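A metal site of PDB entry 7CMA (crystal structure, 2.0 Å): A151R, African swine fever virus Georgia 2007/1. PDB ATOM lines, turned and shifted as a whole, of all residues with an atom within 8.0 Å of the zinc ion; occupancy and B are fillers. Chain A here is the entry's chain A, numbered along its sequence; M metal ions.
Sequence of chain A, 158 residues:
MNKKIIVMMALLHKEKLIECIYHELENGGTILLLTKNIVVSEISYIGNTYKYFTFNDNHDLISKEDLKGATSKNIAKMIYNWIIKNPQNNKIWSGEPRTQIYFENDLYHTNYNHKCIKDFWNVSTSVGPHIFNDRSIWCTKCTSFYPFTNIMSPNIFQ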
ATOM      1  N   TYR A 102      36.156  16.387   6.110  1.00  0.00           N
ATOM      2  CA  TYR A 102      36.180  17.763   5.584  1.00  0.00           C
ATOM      3  C   TYR A 102      35.343  18.664   6.494  1.00  0.00           C
ATOM      4  O   TYR A 102      34.213  18.263   6.842  1.00  0.00           O
ATOM      5  CB  TYR A 102      35.671  17.809   4.139  1.00  0.00           C
ATOM      6  CG  TYR A 102      35.722  19.166   3.490  1.00  0.00           C
ATOM      7  CD1 TYR A 102      36.931  19.767   3.203  1.00  0.00           C
ATOM      8  CD2 TYR A 102      34.567  19.884   3.260  1.00  0.00           C
ATOM      9  CE1 TYR A 102      36.992  21.033   2.624  1.00  0.00           C
ATOM     10  CE2 TYR A 102      34.599  21.150   2.689  1.00  0.00           C
ATOM     11  CZ  TYR A 102      35.821  21.718   2.360  1.00  0.00           C
ATOM     12  OH  TYR A 102      35.856  22.964   1.799  1.00  0.00           O
ATOM     13  N   GLU A 104      33.157  22.082   7.176  1.00  0.00           N
ATOM     14  CA  GLU A 104      32.260  23.050   6.467  1.00  0.00           C
ATOM     15  C   GLU A 104      31.036  23.343   7.339  1.00  0.00           C
ATOM     16  O   GLU A 104      30.477  22.395   7.931  1.00  0.00           O
ATOM     17  CB  GLU A 104      31.833  22.482   5.103  1.00  0.00           C
ATOM     18  CG  GLU A 104      31.715  23.543   4.030  1.00  0.00           C
ATOM     19  CD  GLU A 104      31.061  23.075   2.744  1.00  0.00           C
ATOM     20  OE1 GLU A 104      31.797  22.701   1.807  1.00  0.00           O
ATOM     21  OE2 GLU A 104      29.821  23.109   2.665  1.00  0.00           O
ATOM     22  N   LEU A 107      30.537  22.077  10.990  1.00  0.00           N
ATOM     23  CA  LEU A 107      30.336  20.610  11.113  1.00  0.00           C
ATOM     24  C   LEU A 107      31.468  19.876  10.381  1.00  0.00           C
ATOM     25  O   LEU A 107      32.043  20.465   9.450  1.00  0.00           O
ATOM     26  CB  LEU A 107      28.967  20.252  10.542  1.00  0.00           C
ATOM     27  CG  LEU A 107      27.774  20.548  11.464  1.00  0.00           C
ATOM     28  CD1 LEU A 107      26.464  20.282  10.740  1.00  0.00           C
ATOM     29  CD2 LEU A 107      27.851  19.732  12.741  1.00  0.00           C
ATOM     30  N   TYR A 108      31.846  18.694  10.870  1.00  0.00           N
ATOM     31  CA  TYR A 108      32.834  17.807  10.203  1.00  0.00           C
ATOM     32  C   TYR A 108      32.081  16.712   9.448  1.00  0.00           C
ATOM     33  O   TYR A 108      31.023  16.277   9.955  1.00  0.00           O
ATOM     34  CB  TYR A 108      33.816  17.257  11.243  1.00  0.00           C
ATOM     35  CG  TYR A 108      34.761  18.270  11.820  1.00  0.00           C
ATOM     36  CD1 TYR A 108      34.346  19.158  12.808  1.00  0.00           C
ATOM     37  CD2 TYR A 108      36.055  18.409  11.343  1.00  0.00           C
ATOM     38  CE1 TYR A 108      35.192  20.141  13.299  1.00  0.00           C
ATOM     39  CE2 TYR A 108      36.922  19.355  11.846  1.00  0.00           C
ATOM     40  CZ  TYR A 108      36.495  20.219  12.850  1.00  0.00           C
ATOM     41  OH  TYR A 108      37.319  21.206  13.314  1.00  0.00           O
ATOM     42  N   HIS A 109      32.527  16.419   8.231  1.00  0.00           N
ATOM     43  CA  HIS A 109      31.739  15.538   7.337  1.00  0.00           C
ATOM     44  C   HIS A 109      32.494  14.308   6.863  1.00  0.00           C
ATOM     45  O   HIS A 109      33.709  14.406   6.649  1.00  0.00           O
ATOM     46  CB  HIS A 109      31.288  16.332   6.097  1.00  0.00           C
ATOM     47  CG  HIS A 109      30.546  17.593   6.369  1.00  0.00           C
ATOM     48  ND1 HIS A 109      29.179  17.666   6.317  1.00  0.00           N
ATOM     49  CD2 HIS A 109      30.981  18.839   6.646  1.00  0.00           C
ATOM     50  CE1 HIS A 109      28.802  18.897   6.585  1.00  0.00           C
ATOM     51  NE2 HIS A 109      29.882  19.636   6.785  1.00  0.00           N
ATOM     52  N   THR A 110      31.785  13.201   6.720  1.00  0.00           N
ATOM     53  CA  THR A 110      32.355  11.945   6.161  1.00  0.00           C
ATOM     54  C   THR A 110      31.782  11.713   4.752  1.00  0.00           C
ATOM     55  O   THR A 110      32.379  10.908   4.010  1.00  0.00           O
ATOM     56  CB  THR A 110      32.056  10.749   7.078  1.00  0.00           C
ATOM     57  OG1 THR A 110      30.655  10.775   7.345  1.00  0.00           O
ATOM     58  CG2 THR A 110      32.819  10.788   8.372  1.00  0.00           C
ATOM     59  N   ASN A 111      30.578  12.232   4.493  1.00  0.00           N
ATOM     60  CA  ASN A 111      29.817  12.012   3.239  1.00  0.00           C
ATOM     61  C   ASN A 111      29.341  10.555   3.172  1.00  0.00           C
ATOM     62  O   ASN A 111      29.146  10.063   2.056  1.00  0.00           O
ATOM     63  CB  ASN A 111      30.670  12.360   1.999  1.00  0.00           C
ATOM     64  CG  ASN A 111      30.348  13.726   1.429  1.00  0.00           C
ATOM     65  OD1 ASN A 111      30.081  14.665   2.175  1.00  0.00           O
ATOM     66  ND2 ASN A 111      30.358  13.849   0.106  1.00  0.00           N
ATOM     67  N   TYR A 112      29.251   9.859   4.311  1.00  0.00           N
ATOM     68  CA  TYR A 112      28.851   8.425   4.374  1.00  0.00           C
ATOM     69  C   TYR A 112      27.375   8.283   3.995  1.00  0.00           C
ATOM     70  O   TYR A 112      27.083   7.463   3.122  1.00  0.00           O
ATOM     71  CB  TYR A 112      29.122   7.822   5.758  1.00  0.00           C
ATOM     72  CG  TYR A 112      30.562   7.438   6.017  1.00  0.00           C
ATOM     73  CD1 TYR A 112      31.426   7.161   4.973  1.00  0.00           C
ATOM     74  CD2 TYR A 112      31.062   7.386   7.305  1.00  0.00           C
ATOM     75  CE1 TYR A 112      32.753   6.827   5.203  1.00  0.00           C
ATOM     76  CE2 TYR A 112      32.376   7.021   7.560  1.00  0.00           C
ATOM     77  CZ  TYR A 112      33.221   6.758   6.497  1.00  0.00           C
ATOM     78  OH  TYR A 112      34.527   6.427   6.740  1.00  0.00           O
ATOM     79  N   ASN A 113      26.479   8.974   4.703  1.00  0.00           N
ATOM     80  CA  ASN A 113      25.006   8.738   4.607  1.00  0.00           C
ATOM     81  C   ASN A 113      24.346   9.833   3.770  1.00  0.00           C
ATOM     82  O   ASN A 113      23.119   9.811   3.641  1.00  0.00           O
ATOM     83  CB  ASN A 113      24.334   8.639   5.972  1.00  0.00           C
ATOM     84  CG  ASN A 113      25.031   7.677   6.909  1.00  0.00           C
ATOM     85  OD1 ASN A 113      25.296   8.002   8.063  1.00  0.00           O
ATOM     86  ND2 ASN A 113      25.358   6.490   6.412  1.00  0.00           N
ATOM     87  N   HIS A 114      25.139  10.774   3.242  1.00  0.00           N
ATOM     88  CA  HIS A 114      24.606  11.887   2.402  1.00  0.00           C
ATOM     89  C   HIS A 114      25.805  12.596   1.788  1.00  0.00           C
ATOM     90  O   HIS A 114      26.798  12.789   2.484  1.00  0.00           O
ATOM     91  CB  HIS A 114      23.762  12.868   3.221  1.00  0.00           C
ATOM     92  CG  HIS A 114      23.113  13.943   2.423  1.00  0.00           C
ATOM     93  ND1 HIS A 114      21.844  13.813   1.899  1.00  0.00           N
ATOM     94  CD2 HIS A 114      23.553  15.170   2.066  1.00  0.00           C
ATOM     95  CE1 HIS A 114      21.527  14.912   1.250  1.00  0.00           C
ATOM     96  NE2 HIS A 114      22.556  15.757   1.333  1.00  0.00           N
ATOM     97  N   LYS A 115      25.702  12.969   0.510  1.00  0.00           N
ATOM     98  CA  LYS A 115      26.816  13.665  -0.159  1.00  0.00           C
ATOM     99  C   LYS A 115      26.752  15.153   0.210  1.00  0.00           C
ATOM    100  O   LYS A 115      26.260  15.946  -0.601  1.00  0.00           O
ATOM    101  CB  LYS A 115      26.837  13.409  -1.663  1.00  0.00           C
ATOM    102  CG  LYS A 115      25.500  13.142  -2.338  1.00  0.00           C
ATOM    103  CD  LYS A 115      25.545  13.469  -3.809  1.00  0.00           C
ATOM    104  CE  LYS A 115      26.670  14.430  -4.164  1.00  0.00           C
ATOM    105  NZ  LYS A 115      27.725  13.780  -4.971  1.00  0.00           N
ATOM    106  N   CYS A 116      27.218  15.488   1.409  1.00  0.00           N
ATOM    107  CA  CYS A 116      27.204  16.889   1.884  1.00  0.00           C
ATOM    108  C   CYS A 116      28.286  17.682   1.134  1.00  0.00           C
ATOM    109  O   CYS A 116      28.046  18.856   0.842  1.00  0.00           O
ATOM    110  CB  CYS A 116      27.501  16.896   3.367  1.00  0.00           C
ATOM    111  SG  CYS A 116      26.084  16.478   4.429  1.00  0.00           S
ATOM    112  N   ILE A 117      29.405  17.033   0.806  1.00  0.00           N
ATOM    113  CA  ILE A 117      30.567  17.739   0.196  1.00  0.00           C
ATOM    114  C   ILE A 117      30.821  17.260  -1.239  1.00  0.00           C
ATOM    115  O   ILE A 117      30.777  16.054  -1.464  1.00  0.00           O
ATOM    116  CB  ILE A 117      31.803  17.544   1.086  1.00  0.00           C
ATOM    117  CG1 ILE A 117      31.531  17.880   2.550  1.00  0.00           C
ATOM    118  CG2 ILE A 117      32.990  18.313   0.538  1.00  0.00           C
ATOM    119  CD1 ILE A 117      31.041  19.288   2.783  1.00  0.00           C
ATOM    120  N   PHE A 120      34.661  15.683  -2.675  1.00  0.00           N
ATOM    121  CA  PHE A 120      35.049  15.297  -1.289  1.00  0.00           C
ATOM    122  C   PHE A 120      36.382  14.547  -1.316  1.00  0.00           C
ATOM    123  O   PHE A 120      37.259  14.838  -0.482  1.00  0.00           O
ATOM    124  CB  PHE A 120      33.947  14.441  -0.656  1.00  0.00           C
ATOM    125  CG  PHE A 120      34.251  13.948   0.740  1.00  0.00           C
ATOM    126  CD1 PHE A 120      34.147  14.806   1.824  1.00  0.00           C
ATOM    127  CD2 PHE A 120      34.663  12.652   0.964  1.00  0.00           C
ATOM    128  CE1 PHE A 120      34.421  14.361   3.106  1.00  0.00           C
ATOM    129  CE2 PHE A 120      34.952  12.203   2.247  1.00  0.00           C
ATOM    130  CZ  PHE A 120      34.826  13.068   3.319  1.00  0.00           C
ATOM    131  N   TRP A 138      30.114  16.258  14.719  1.00  0.00           N
ATOM    132  CA  TRP A 138      29.901  15.504  13.455  1.00  0.00           C
ATOM    133  C   TRP A 138      28.529  15.780  12.821  1.00  0.00           C
ATOM    134  O   TRP A 138      27.536  15.791  13.544  1.00  0.00           O
ATOM    135  CB  TRP A 138      30.188  14.024  13.666  1.00  0.00           C
ATOM    136  CG  TRP A 138      31.635  13.812  13.963  1.00  0.00           C
ATOM    137  CD1 TRP A 138      32.228  13.675  15.188  1.00  0.00           C
ATOM    138  CD2 TRP A 138      32.699  13.806  12.996  1.00  0.00           C
ATOM    139  NE1 TRP A 138      33.586  13.565  15.041  1.00  0.00           N
ATOM    140  CE2 TRP A 138      33.897  13.639  13.713  1.00  0.00           C
ATOM    141  CE3 TRP A 138      32.748  13.893  11.606  1.00  0.00           C
ATOM    142  CZ2 TRP A 138      35.128  13.575  13.080  1.00  0.00           C
ATOM    143  CZ3 TRP A 138      33.964  13.826  10.980  1.00  0.00           C
ATOM    144  CH2 TRP A 138      35.146  13.678  11.713  1.00  0.00           C
ATOM    145  N   CYS A 139      28.507  15.983  11.497  1.00  0.00           N
ATOM    146  CA  CYS A 139      27.256  16.270  10.744  1.00  0.00           C
ATOM    147  C   CYS A 139      26.287  15.094  10.861  1.00  0.00           C
ATOM    148  O   CYS A 139      26.684  13.990  10.507  1.00  0.00           O
ATOM    149  CB  CYS A 139      27.612  16.555   9.289  1.00  0.00           C
ATOM    150  SG  CYS A 139      26.208  16.670   8.146  1.00  0.00           S
ATOM    151  N   THR A 140      25.065  15.349  11.316  1.00  0.00           N
ATOM    152  CA  THR A 140      24.093  14.255  11.576  1.00  0.00           C
ATOM    153  C   THR A 140      23.449  13.773  10.280  1.00  0.00           C
ATOM    154  O   THR A 140      22.718  12.781  10.335  1.00  0.00           O
ATOM    155  CB  THR A 140      23.001  14.758  12.515  1.00  0.00           C
ATOM    156  OG1 THR A 140      22.289  15.790  11.842  1.00  0.00           O
ATOM    157  CG2 THR A 140      23.542  15.263  13.827  1.00  0.00           C
ATOM    158  N   LYS A 141      23.706  14.466   9.168  1.00  0.00           N
ATOM    159  CA  LYS A 141      23.117  14.091   7.870  1.00  0.00           C
ATOM    160  C   LYS A 141      23.998  13.060   7.176  1.00  0.00           C
ATOM    161  O   LYS A 141      23.454  12.141   6.592  1.00  0.00           O
ATOM    162  CB  LYS A 141      22.948  15.331   6.980  1.00  0.00           C
ATOM    163  CG  LYS A 141      22.155  16.466   7.593  1.00  0.00           C
ATOM    164  CD  LYS A 141      21.662  17.447   6.558  1.00  0.00           C
ATOM    165  CE  LYS A 141      21.971  17.011   5.145  1.00  0.00           C
ATOM    166  NZ  LYS A 141      21.367  17.918   4.144  1.00  0.00           N
ATOM    167  N   CYS A 142      25.314  13.222   7.259  1.00  0.00           N
ATOM    168  CA  CYS A 142      26.227  12.301   6.535  1.00  0.00           C
ATOM    169  C   CYS A 142      26.956  11.352   7.490  1.00  0.00           C
ATOM    170  O   CYS A 142      27.518  10.382   7.001  1.00  0.00           O
ATOM    171  CB  CYS A 142      27.238  13.081   5.705  1.00  0.00           C
ATOM    172  SG  CYS A 142      28.319  14.176   6.656  1.00  0.00           S
ATOM    173  N   THR A 143      26.960  11.656   8.783  1.00  0.00           N
ATOM    174  CA  THR A 143      27.756  10.830   9.727  1.00  0.00           C
ATOM    175  C   THR A 143      26.831  10.219  10.782  1.00  0.00           C
ATOM    176  O   THR A 143      26.244  10.967  11.569  1.00  0.00           O
ATOM    177  CB  THR A 143      28.948  11.603  10.293  1.00  0.00           C
ATOM    178  OG1 THR A 143      29.575  12.340   9.246  1.00  0.00           O
ATOM    179  CG2 THR A 143      29.965  10.716  10.988  1.00  0.00           C
HETATM  180 ZN    ZN M   1      27.470  16.236   6.206  1.00  0.00          ZN
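Four residues have an atom within 4 Å of the zinc ion: His 109, Cys 116, Cys 139 and Cys 142. The nearest printed residue that does not touch the zinc ion is Lys 141 (4.7 Å).
The zinc ion is bound by a ring nitrogen (ND1) of His 109, the side-chain sulfur of Cys 116, the side-chain sulfur of Cys 142 and the side-chain sulfur of Cys 139.
The backbone NH (N) of His 109 sits at hydrogen-bond distance from the backbone carbonyl oxygen (O) of Tyr 102, 2.9 Å away. OD1 of Asn 111 sits at hydrogen-bond distance from N of Cys 116 (3.1 Å). The side-chain sulfur (SG) of Cys 142 sits close to the backbone NH (N) of Asn 111, at 3.7 Å. The side-chain sulfur of Cys 142 lies close to the side-chain hydroxyl of Thr 143 (3.4 Å). The backbone carbonyl oxygen (O) of Cys 142 lies within hydrogen-bond range of the side-chain hydroxyl (OG1) of Thr 110 (3.2 Å). O of Cys 142 is in hydrogen-bond range of N of Tyr 112, at 3.2 Å. The backbone NH of Asn 113 lies within hydrogen-bond range of the backbone carbonyl oxygen of Cys 142 (2.9 Å). N of Cys 139 sits at hydrogen-bond distance from O of Tyr 108.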
